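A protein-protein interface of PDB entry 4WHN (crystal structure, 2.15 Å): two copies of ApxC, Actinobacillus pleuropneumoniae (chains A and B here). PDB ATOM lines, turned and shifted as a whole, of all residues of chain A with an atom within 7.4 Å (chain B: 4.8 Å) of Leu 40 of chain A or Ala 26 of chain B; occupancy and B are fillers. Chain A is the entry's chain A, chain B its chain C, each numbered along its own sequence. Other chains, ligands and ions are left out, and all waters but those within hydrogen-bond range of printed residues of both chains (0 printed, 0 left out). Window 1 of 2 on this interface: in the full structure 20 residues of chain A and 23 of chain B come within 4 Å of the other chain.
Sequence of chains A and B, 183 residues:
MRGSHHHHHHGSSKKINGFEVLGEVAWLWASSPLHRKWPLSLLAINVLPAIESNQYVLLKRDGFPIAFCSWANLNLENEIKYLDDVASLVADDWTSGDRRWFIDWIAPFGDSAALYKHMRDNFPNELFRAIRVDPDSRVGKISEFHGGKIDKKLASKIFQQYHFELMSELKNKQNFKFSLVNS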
ATOM      1  N   PHE A  19      19.871   7.638  32.099  1.00  0.00           N
ATOM      2  CA  PHE A  19      19.938   7.070  30.758  1.00  0.00           C
ATOM      3  C   PHE A  19      20.009   5.579  30.810  1.00  0.00           C
ATOM      4  O   PHE A  19      19.426   4.889  29.984  1.00  0.00           O
ATOM      5  CB  PHE A  19      21.157   7.619  30.010  1.00  0.00           C
ATOM      6  CG  PHE A  19      20.973   9.013  29.499  1.00  0.00           C
ATOM      7  CD1 PHE A  19      19.895   9.322  28.660  1.00  0.00           C
ATOM      8  CD2 PHE A  19      21.898  10.015  29.797  1.00  0.00           C
ATOM      9  CE1 PHE A  19      19.711  10.617  28.183  1.00  0.00           C
ATOM     10  CE2 PHE A  19      21.742  11.282  29.268  1.00  0.00           C
ATOM     11  CZ  PHE A  19      20.645  11.589  28.466  1.00  0.00           C
ATOM     12  N   LEU A  22      16.571   4.445  31.484  1.00  0.00           N
ATOM     13  CA  LEU A  22      15.756   4.647  30.303  1.00  0.00           C
ATOM     14  C   LEU A  22      16.048   3.571  29.224  1.00  0.00           C
ATOM     15  O   LEU A  22      15.135   3.052  28.572  1.00  0.00           O
ATOM     16  CB  LEU A  22      16.038   6.027  29.759  1.00  0.00           C
ATOM     17  CG  LEU A  22      15.264   6.366  28.501  1.00  0.00           C
ATOM     18  CD1 LEU A  22      13.785   6.421  28.767  1.00  0.00           C
ATOM     19  CD2 LEU A  22      15.744   7.700  27.957  1.00  0.00           C
ATOM     20  N   GLY A  23      17.314   3.177  29.099  1.00  0.00           N
ATOM     21  CA  GLY A  23      17.700   2.117  28.141  1.00  0.00           C
ATOM     22  C   GLY A  23      17.128   0.763  28.539  1.00  0.00           C
ATOM     23  O   GLY A  23      16.610   0.009  27.710  1.00  0.00           O
ATOM     24  N   ALA A  26      13.476   0.858  27.727  1.00  0.00           N
ATOM     25  CA  ALA A  26      13.273   0.797  26.292  1.00  0.00           C
ATOM     26  C   ALA A  26      13.447  -0.618  25.795  1.00  0.00           C
ATOM     27  O   ALA A  26      12.677  -1.094  24.933  1.00  0.00           O
ATOM     28  CB  ALA A  26      14.275   1.709  25.605  1.00  0.00           C
ATOM     29  N   TRP A  29      10.425  -2.524  26.686  1.00  0.00           N
ATOM     30  CA  TRP A  29       9.302  -2.275  25.759  1.00  0.00           C
ATOM     31  C   TRP A  29       9.490  -3.039  24.446  1.00  0.00           C
ATOM     32  O   TRP A  29       8.530  -3.545  23.846  1.00  0.00           O
ATOM     33  CB  TRP A  29       9.193  -0.769  25.437  1.00  0.00           C
ATOM     34  CG  TRP A  29       8.535   0.114  26.484  1.00  0.00           C
ATOM     35  CD1 TRP A  29       8.615  -0.027  27.819  1.00  0.00           C
ATOM     36  CD2 TRP A  29       7.765   1.298  26.252  1.00  0.00           C
ATOM     37  NE1 TRP A  29       7.947   0.990  28.454  1.00  0.00           N
ATOM     38  CE2 TRP A  29       7.403   1.817  27.516  1.00  0.00           C
ATOM     39  CE3 TRP A  29       7.380   1.978  25.121  1.00  0.00           C
ATOM     40  CZ2 TRP A  29       6.666   2.964  27.670  1.00  0.00           C
ATOM     41  CZ3 TRP A  29       6.607   3.118  25.274  1.00  0.00           C
ATOM     42  CH2 TRP A  29       6.265   3.601  26.523  1.00  0.00           C
ATOM     43  N   LYS A  37       5.419  -1.671  19.632  1.00  0.00           N
ATOM     44  CA  LYS A  37       4.827  -0.910  18.576  1.00  0.00           C
ATOM     45  C   LYS A  37       4.610   0.571  18.960  1.00  0.00           C
ATOM     46  O   LYS A  37       4.280   1.366  18.136  1.00  0.00           O
ATOM     47  CB  LYS A  37       3.495  -1.515  18.193  1.00  0.00           C
ATOM     48  CG  LYS A  37       3.610  -2.986  17.851  1.00  0.00           C
ATOM     49  CD  LYS A  37       2.315  -3.525  17.309  1.00  0.00           C
ATOM     50  CE  LYS A  37       2.568  -4.382  16.108  1.00  0.00           C
ATOM     51  NZ  LYS A  37       1.507  -5.410  15.958  1.00  0.00           N
ATOM     52  N   TRP A  38       4.784   0.920  20.208  1.00  0.00           N
ATOM     53  CA  TRP A  38       4.534   2.276  20.616  1.00  0.00           C
ATOM     54  C   TRP A  38       5.737   3.150  20.204  1.00  0.00           C
ATOM     55  O   TRP A  38       6.844   2.674  20.090  1.00  0.00           O
ATOM     56  CB  TRP A  38       4.333   2.303  22.115  1.00  0.00           C
ATOM     57  CG  TRP A  38       3.080   1.631  22.563  1.00  0.00           C
ATOM     58  CD1 TRP A  38       2.213   0.908  21.813  1.00  0.00           C
ATOM     59  CD2 TRP A  38       2.578   1.595  23.891  1.00  0.00           C
ATOM     60  NE1 TRP A  38       1.195   0.429  22.586  1.00  0.00           N
ATOM     61  CE2 TRP A  38       1.396   0.821  23.871  1.00  0.00           C
ATOM     62  CE3 TRP A  38       3.002   2.156  25.095  1.00  0.00           C
ATOM     63  CZ2 TRP A  38       0.611   0.606  25.009  1.00  0.00           C
ATOM     64  CZ3 TRP A  38       2.239   1.900  26.251  1.00  0.00           C
ATOM     65  CH2 TRP A  38       1.057   1.147  26.191  1.00  0.00           C
ATOM     66  N   PRO A  39       5.513   4.451  20.050  1.00  0.00           N
ATOM     67  CA  PRO A  39       6.552   5.320  19.588  1.00  0.00           C
ATOM     68  C   PRO A  39       7.511   5.755  20.666  1.00  0.00           C
ATOM     69  O   PRO A  39       7.188   5.785  21.862  1.00  0.00           O
ATOM     70  CB  PRO A  39       5.759   6.484  18.973  1.00  0.00           C
ATOM     71  CG  PRO A  39       4.490   6.535  19.798  1.00  0.00           C
ATOM     72  CD  PRO A  39       4.175   5.103  20.085  1.00  0.00           C
ATOM     73  N   LEU A  40       8.699   6.147  20.222  1.00  0.00           N
ATOM     74  CA  LEU A  40       9.667   6.733  21.113  1.00  0.00           C
ATOM     75  C   LEU A  40       9.161   7.968  21.882  1.00  0.00           C
ATOM     76  O   LEU A  40       9.534   8.185  23.051  1.00  0.00           O
ATOM     77  CB  LEU A  40      10.949   7.154  20.391  1.00  0.00           C
ATOM     78  CG  LEU A  40      12.100   6.119  20.301  1.00  0.00           C
ATOM     79  CD1 LEU A  40      12.625   5.832  21.669  1.00  0.00           C
ATOM     80  CD2 LEU A  40      11.717   4.870  19.554  1.00  0.00           C
ATOM     81  N   SER A  41       8.334   8.779  21.244  1.00  0.00           N
ATOM     82  CA  SER A  41       7.711   9.921  21.952  1.00  0.00           C
ATOM     83  C   SER A  41       6.981   9.461  23.230  1.00  0.00           C
ATOM     84  O   SER A  41       6.998  10.170  24.223  1.00  0.00           O
ATOM     85  CB  SER A  41       6.685  10.649  21.061  1.00  0.00           C
ATOM     86  OG  SER A  41       5.665   9.752  20.613  1.00  0.00           O
ATOM     87  N   LEU A  42       6.270   8.341  23.162  1.00  0.00           N
ATOM     88  CA  LEU A  42       5.527   7.830  24.326  1.00  0.00           C
ATOM     89  C   LEU A  42       6.427   7.268  25.385  1.00  0.00           C
ATOM     90  O   LEU A  42       6.144   7.358  26.587  1.00  0.00           O
ATOM     91  CB  LEU A  42       4.527   6.779  23.899  1.00  0.00           C
ATOM     92  CG  LEU A  42       3.445   6.399  24.925  1.00  0.00           C
ATOM     93  CD1 LEU A  42       2.766   7.659  25.490  1.00  0.00           C
ATOM     94  CD2 LEU A  42       2.388   5.503  24.312  1.00  0.00           C
ATOM     95  N   LEU A  43       7.520   6.665  24.968  1.00  0.00           N
ATOM     96  CA  LEU A  43       8.519   6.267  25.910  1.00  0.00           C
ATOM     97  C   LEU A  43       9.011   7.488  26.708  1.00  0.00           C
ATOM     98  O   LEU A  43       9.146   7.438  27.944  1.00  0.00           O
ATOM     99  CB  LEU A  43       9.728   5.622  25.194  1.00  0.00           C
ATOM    100  CG  LEU A  43      10.836   5.159  26.145  1.00  0.00           C
ATOM    101  CD1 LEU A  43      10.459   3.810  26.680  1.00  0.00           C
ATOM    102  CD2 LEU A  43      12.212   5.115  25.487  1.00  0.00           C
ATOM    103  N   ALA A  44       9.402   8.553  26.035  1.00  0.00           N
ATOM    104  CA  ALA A  44       9.855   9.784  26.765  1.00  0.00           C
ATOM    105  C   ALA A  44       8.779  10.339  27.689  1.00  0.00           C
ATOM    106  O   ALA A  44       9.010  10.569  28.848  1.00  0.00           O
ATOM    107  CB  ALA A  44      10.282  10.873  25.805  1.00  0.00           C
ATOM    108  N   ILE A  45       7.563  10.434  27.184  1.00  0.00           N
ATOM    109  CA  ILE A  45       6.435  10.923  28.005  1.00  0.00           C
ATOM    110  C   ILE A  45       6.164  10.083  29.259  1.00  0.00           C
ATOM    111  O   ILE A  45       5.964  10.611  30.338  1.00  0.00           O
ATOM    112  CB  ILE A  45       5.190  10.993  27.133  1.00  0.00           C
ATOM    113  CG1 ILE A  45       5.301  12.274  26.257  1.00  0.00           C
ATOM    114  CG2 ILE A  45       3.921  11.039  27.974  1.00  0.00           C
ATOM    115  CD1 ILE A  45       4.286  12.307  25.138  1.00  0.00           C
ATOM    116  N   ASN A  46       6.156   8.773  29.100  1.00  0.00           N
ATOM    117  CA  ASN A  46       5.795   7.873  30.199  1.00  0.00           C
ATOM    118  C   ASN A  46       6.949   7.639  31.138  1.00  0.00           C
ATOM    119  O   ASN A  46       6.742   7.358  32.323  1.00  0.00           O
ATOM    120  CB  ASN A  46       5.395   6.493  29.696  1.00  0.00           C
ATOM    121  CG  ASN A  46       4.003   6.394  29.185  1.00  0.00           C
ATOM    122  OD1 ASN A  46       3.523   5.266  28.860  1.00  0.00           O
ATOM    123  ND2 ASN A  46       3.299   7.474  29.178  1.00  0.00           N
ATOM    124  N   LEU B  22      22.054   2.929  24.990  1.00  0.00           N
ATOM    125  CA  LEU B  22      20.754   2.741  24.395  1.00  0.00           C
ATOM    126  C   LEU B  22      19.781   3.850  24.863  1.00  0.00           C
ATOM    127  O   LEU B  22      18.939   4.332  24.088  1.00  0.00           O
ATOM    128  CB  LEU B  22      20.202   1.377  24.763  1.00  0.00           C
ATOM    129  CG  LEU B  22      18.815   1.040  24.198  1.00  0.00           C
ATOM    130  CD1 LEU B  22      18.787   0.993  22.682  1.00  0.00           C
ATOM    131  CD2 LEU B  22      18.325  -0.264  24.750  1.00  0.00           C
ATOM    132  N   GLY B  23      19.881   4.229  26.141  1.00  0.00           N
ATOM    133  CA  GLY B  23      19.008   5.252  26.738  1.00  0.00           C
ATOM    134  C   GLY B  23      19.277   6.596  26.116  1.00  0.00           C
ATOM    135  O   GLY B  23      18.360   7.334  25.728  1.00  0.00           O
ATOM    136  N   GLU B  24      20.538   6.892  25.936  1.00  0.00           N
ATOM    137  CA  GLU B  24      20.896   8.142  25.270  1.00  0.00           C
ATOM    138  C   GLU B  24      20.359   8.199  23.887  1.00  0.00           C
ATOM    139  O   GLU B  24      19.799   9.188  23.477  1.00  0.00           O
ATOM    140  CB  GLU B  24      22.413   8.334  25.241  1.00  0.00           C
ATOM    141  CG  GLU B  24      22.927   8.646  26.633  1.00  0.00           C
ATOM    142  CD  GLU B  24      24.316   9.262  26.716  1.00  0.00           C
ATOM    143  OE1 GLU B  24      25.075   8.864  27.598  1.00  0.00           O
ATOM    144  OE2 GLU B  24      24.648  10.193  25.950  1.00  0.00           O
ATOM    145  N   VAL B  25      20.510   7.127  23.144  1.00  0.00           N
ATOM    146  CA  VAL B  25      20.034   7.116  21.745  1.00  0.00           C
ATOM    147  C   VAL B  25      18.522   7.221  21.691  1.00  0.00           C
ATOM    148  O   VAL B  25      18.002   7.972  20.894  1.00  0.00           O
ATOM    149  CB  VAL B  25      20.504   5.852  20.957  1.00  0.00           C
ATOM    150  CG1 VAL B  25      19.917   5.829  19.530  1.00  0.00           C
ATOM    151  CG2 VAL B  25      22.001   5.912  20.866  1.00  0.00           C
ATOM    152  N   ALA B  26      17.838   6.513  22.583  1.00  0.00           N
ATOM    153  CA  ALA B  26      16.384   6.636  22.689  1.00  0.00           C
ATOM    154  C   ALA B  26      15.956   8.083  22.936  1.00  0.00           C
ATOM    155  O   ALA B  26      15.034   8.579  22.328  1.00  0.00           O
ATOM    156  CB  ALA B  26      15.853   5.729  23.788  1.00  0.00           C
ATOM    157  N   TRP B  27      16.675   8.760  23.823  1.00  0.00           N
ATOM    158  CA  TRP B  27      16.343  10.138  24.171  1.00  0.00           C
ATOM    159  C   TRP B  27      16.555  11.021  22.979  1.00  0.00           C
ATOM    160  O   TRP B  27      15.739  11.882  22.652  1.00  0.00           O
ATOM    161  CB  TRP B  27      17.219  10.571  25.327  1.00  0.00           C
ATOM    162  CG  TRP B  27      16.920  11.916  25.810  1.00  0.00           C
ATOM    163  CD1 TRP B  27      16.027  12.267  26.788  1.00  0.00           C
ATOM    164  CD2 TRP B  27      17.552  13.115  25.400  1.00  0.00           C
ATOM    165  NE1 TRP B  27      16.049  13.634  26.966  1.00  0.00           N
ATOM    166  CE2 TRP B  27      16.972  14.174  26.129  1.00  0.00           C
ATOM    167  CE3 TRP B  27      18.547  13.406  24.474  1.00  0.00           C
ATOM    168  CZ2 TRP B  27      17.359  15.509  25.957  1.00  0.00           C
ATOM    169  CZ3 TRP B  27      18.926  14.729  24.284  1.00  0.00           C
ATOM    170  CH2 TRP B  27      18.334  15.770  25.041  1.00  0.00           C
ATOM    171  N   LEU B  28      17.627  10.759  22.255  1.00  0.00           N
ATOM    172  CA  LEU B  28      17.895  11.530  21.050  1.00  0.00           C
ATOM    173  C   LEU B  28      16.916  11.262  19.971  1.00  0.00           C
ATOM    174  O   LEU B  28      16.521  12.208  19.323  1.00  0.00           O
ATOM    175  CB  LEU B  28      19.330  11.338  20.621  1.00  0.00           C
ATOM    176  CG  LEU B  28      19.936  12.261  19.584  1.00  0.00           C
ATOM    177  CD1 LEU B  28      20.009  13.706  20.121  1.00  0.00           C
ATOM    178  CD2 LEU B  28      21.344  11.732  19.326  1.00  0.00           C
ATOM    179  N   TRP B  29      16.447  10.014  19.794  1.00  0.00           N
ATOM    180  CA  TRP B  29      15.354   9.742  18.838  1.00  0.00           C
ATOM    181  C   TRP B  29      14.095  10.531  19.247  1.00  0.00           C
ATOM    182  O   TRP B  29      13.390  11.106  18.418  1.00  0.00           O
ATOM    183  CB  TRP B  29      14.987   8.278  18.790  1.00  0.00           C
ATOM    184  CG  TRP B  29      15.853   7.408  17.998  1.00  0.00           C
ATOM    185  CD1 TRP B  29      17.194   7.525  17.806  1.00  0.00           C
ATOM    186  CD2 TRP B  29      15.444   6.231  17.270  1.00  0.00           C
ATOM    187  NE1 TRP B  29      17.653   6.488  17.025  1.00  0.00           N
ATOM    188  CE2 TRP B  29      16.601   5.690  16.666  1.00  0.00           C
ATOM    189  CE3 TRP B  29      14.225   5.571  17.093  1.00  0.00           C
ATOM    190  CZ2 TRP B  29      16.554   4.539  15.878  1.00  0.00           C
ATOM    191  CZ3 TRP B  29      14.183   4.453  16.308  1.00  0.00           C
ATOM    192  CH2 TRP B  29      15.334   3.933  15.731  1.00  0.00           C
ATOM    193  N   ALA B  30      13.814  10.544  20.548  1.00  0.00           N
ATOM    194  CA  ALA B  30      12.625  11.233  21.088  1.00  0.00           C
ATOM    195  C   ALA B  30      12.713  12.751  20.917  1.00  0.00           C
ATOM    196  O   ALA B  30      11.692  13.423  20.903  1.00  0.00           O
ATOM    197  CB  ALA B  30      12.403  10.882  22.555  1.00  0.00           C
ATOM    198  N   HIS B  35      12.224  10.595  13.977  1.00  0.00           N
ATOM    199  CA  HIS B  35      12.521   9.369  14.735  1.00  0.00           C
ATOM    200  C   HIS B  35      11.625   9.215  15.966  1.00  0.00           C
ATOM    201  O   HIS B  35      11.371   8.112  16.398  1.00  0.00           O
ATOM    202  CB  HIS B  35      13.969   9.311  15.190  1.00  0.00           C
ATOM    203  CG  HIS B  35      14.917   8.834  14.128  1.00  0.00           C
ATOM    204  ND1 HIS B  35      15.314   9.638  13.075  1.00  0.00           N
ATOM    205  CD2 HIS B  35      15.564   7.656  13.958  1.00  0.00           C
ATOM    206  CE1 HIS B  35      16.177   8.989  12.319  1.00  0.00           C
ATOM    207  NE2 HIS B  35      16.345   7.779  12.829  1.00  0.00           N
ATOM    208  N   ARG B  36      11.132  10.310  16.518  1.00  0.00           N
ATOM    209  CA  ARG B  36      10.294  10.222  17.712  1.00  0.00           C
ATOM    210  C   ARG B  36       9.043   9.494  17.428  1.00  0.00           C
ATOM    211  O   ARG B  36       8.375   9.041  18.356  1.00  0.00           O
ATOM    212  CB  ARG B  36       9.938  11.584  18.290  1.00  0.00           C
ATOM    213  CG  ARG B  36       9.018  12.421  17.403  1.00  0.00           C
ATOM    214  CD  ARG B  36       8.993  13.890  17.881  1.00  0.00           C
ATOM    215  NE  ARG B  36       8.079  13.925  19.002  1.00  0.00           N
ATOM    216  CZ  ARG B  36       6.741  13.924  18.894  1.00  0.00           C
ATOM    217  NH1 ARG B  36       6.131  14.003  17.706  1.00  0.00           N
ATOM    218  NH2 ARG B  36       6.005  13.893  19.992  1.00  0.00           N
ATOM    219  N   TRP B  38       8.925   6.779  15.517  1.00  0.00           N
ATOM    220  CA  TRP B  38       9.209   5.421  15.136  1.00  0.00           C
ATOM    221  C   TRP B  38       8.972   4.523  16.334  1.00  0.00           C
ATOM    222  O   TRP B  38       9.045   4.989  17.444  1.00  0.00           O
ATOM    223  CB  TRP B  38      10.635   5.325  14.640  1.00  0.00           C
ATOM    224  CG  TRP B  38      10.864   6.027  13.345  1.00  0.00           C
ATOM    225  CD1 TRP B  38       9.989   6.760  12.660  1.00  0.00           C
ATOM    226  CD2 TRP B  38      12.079   6.033  12.586  1.00  0.00           C
ATOM    227  NE1 TRP B  38      10.564   7.216  11.492  1.00  0.00           N
ATOM    228  CE2 TRP B  38      11.847   6.779  11.433  1.00  0.00           C
ATOM    229  CE3 TRP B  38      13.303   5.408  12.735  1.00  0.00           C
ATOM    230  CZ2 TRP B  38      12.832   6.991  10.453  1.00  0.00           C
ATOM    231  CZ3 TRP B  38      14.274   5.610  11.781  1.00  0.00           C
ATOM    232  CH2 TRP B  38      14.040   6.405  10.652  1.00  0.00           C
ATOM    233  N   PRO B  39       8.670   3.242  16.096  1.00  0.00           N
ATOM    234  CA  PRO B  39       8.394   2.318  17.156  1.00  0.00           C
ATOM    235  C   PRO B  39       9.602   1.760  17.876  1.00  0.00           C
ATOM    236  O   PRO B  39      10.762   1.806  17.398  1.00  0.00           O
ATOM    237  CB  PRO B  39       7.633   1.219  16.462  1.00  0.00           C
ATOM    238  CG  PRO B  39       8.234   1.208  15.082  1.00  0.00           C
ATOM    239  CD  PRO B  39       8.504   2.621  14.761  1.00  0.00           C
ATOM    240  N   LEU B  40       9.362   1.362  19.121  1.00  0.00           N
ATOM    241  CA  LEU B  40      10.433   0.836  19.939  1.00  0.00           C
ATOM    242  C   LEU B  40      11.073  -0.392  19.280  1.00  0.00           C
ATOM    243  O   LEU B  40      12.301  -0.638  19.500  1.00  0.00           O
ATOM    244  CB  LEU B  40       9.952   0.464  21.355  1.00  0.00           C
ATOM    245  CG  LEU B  40      10.117   1.470  22.484  1.00  0.00           C
ATOM    246  CD1 LEU B  40      11.595   1.721  22.777  1.00  0.00           C
ATOM    247  CD2 LEU B  40       9.376   2.798  22.229  1.00  0.00           C
ATOM    248  N   LEU B  43      13.906   0.857  17.224  1.00  0.00           N
ATOM    249  CA  LEU B  43      15.029   1.229  18.022  1.00  0.00           C
ATOM    250  C   LEU B  43      15.883  -0.023  18.331  1.00  0.00           C
ATOM    251  O   LEU B  43      17.096   0.030  18.213  1.00  0.00           O
ATOM    252  CB  LEU B  43      14.571   1.853  19.338  1.00  0.00           C
ATOM    253  CG  LEU B  43      15.702   2.300  20.275  1.00  0.00           C
ATOM    254  CD1 LEU B  43      16.200   3.664  19.827  1.00  0.00           C
ATOM    255  CD2 LEU B  43      15.273   2.358  21.719  1.00  0.00           C
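The backbone carbonyl oxygen (O) of Trp 29 of chain B sits at hydrogen-bond distance from the backbone NH (N) of Arg 36 of chain B, at 3.1 Å.
Among the printed residues, merely in contact across the chains: Phe 19 of chain A with Gly 23 of chain B (3.3 Å), Pro 39 of chain A with Trp 38 of chain B (3.3 Å), Trp 38 of chain A with Pro 39 of chain B (3.3 Å), Gly 23 of chain A with Leu 22 of chain B (3.4 Å), Leu 22 of chain A with Gly 23 of chain B (3.5 Å), Phe 19 of chain A with Glu 24 of chain B (3.5 Å), Gly 23 of chain A with Gly 23 of chain B (3.6 Å), Leu 40 of chain A with Trp 29 of chain B (3.6 Å), Trp 29 of chain A with Leu 40 of chain B (3.6 Å), Ala 26 of chain A with Leu 40 of chain B (3.7 Å), Pro 39 of chain A with Arg 36 of chain B (3.7 Å), Leu 40 of chain A with Ala 26 of chain B (3.7 Å), Pro 39 of chain A with Leu 40 of chain B (3.7 Å), Lys 37 of chain A with Pro 39 of chain B (3.8 Å), Phe 19 of chain A with Trp 27 of chain B (3.8 Å), Leu 40 of chain A with Pro 39 of chain B (3.9 Å), Ala 44 of chain A with Ala 30 of chain B (3.9 Å), Leu 40 of chain A with Leu 40 of chain B (3.96 Å) and Leu 40 of chain A with Ala 30 of chain B (3.97 Å).
Among the printed residues, 23 pairs touch across the chains. Among the printed residues, no Asp or Glu carboxylate lies within 4 Å of a Lys or Arg side-chain nitrogen of the other chain.
Gly 23 of chain A touches its own counterpart, Gly 23 of chain B. Ala 26 of chain A touches Leu 40 of chain B, and with the chains exchanged Leu 40 of chain A touches Ala 26 of chain B. Pro 39 of chain A touches Leu 40 of chain B, and with the chains exchanged Leu 40 of chain A touches Pro 39 of chain B. Leu 40 of chain A touches its own counterpart, Leu 40 of chain B. 8 positions are printed for both chains. Of the 23 pairs that touch across the chains among the printed residues, 14 have their exchanged pair printed and touching as well.
The backbone NH of Leu 40 of chain B is in hydrogen-bond range of the backbone carbonyl oxygen of Trp 38 of chain A (3.0 Å). The backbone NH (N) of Leu 40 of chain A is in hydrogen-bond range of the backbone carbonyl oxygen (O) of Arg 36 of chain B (3.5 Å). The backbone NH (N) of Leu 40 of chain A is in hydrogen-bond range of the backbone carbonyl oxygen (O) of Trp 38 of chain B, 3.0 Å away. The backbone NH (N) of Ser 41 of chain A sits at hydrogen-bond distance from the backbone carbonyl oxygen (O) of Arg 36 of chain B.
Printed residues of chain B within 4 Å of Phe 19 of chain A: Gly 23 (3.3 Å), Glu 24 (3.5 Å) and Trp 27 (3.8 Å). Of chain B, only Ala 26, Trp 29, Ala 30, Arg 36, Trp 38, Pro 39 and Leu 40 come within 4 Å of Leu 40 of chain A. Printed residues of chain A within 4 Å of Leu 22 of chain B: Gly 23 (3.4 Å). Of the printed residues of chain A, Gly 23 of chain B touches Phe 19 (3.3 Å), Leu 22 (3.5 Å) and Gly 23 (3.6 Å). Of chain A, only Leu 40 comes within 4 Å of Ala 26 of chain B. His 35 of chain B touches none of the printed residues of chain A. Leu 43 of chain B touches none of the printed residues of chain A.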
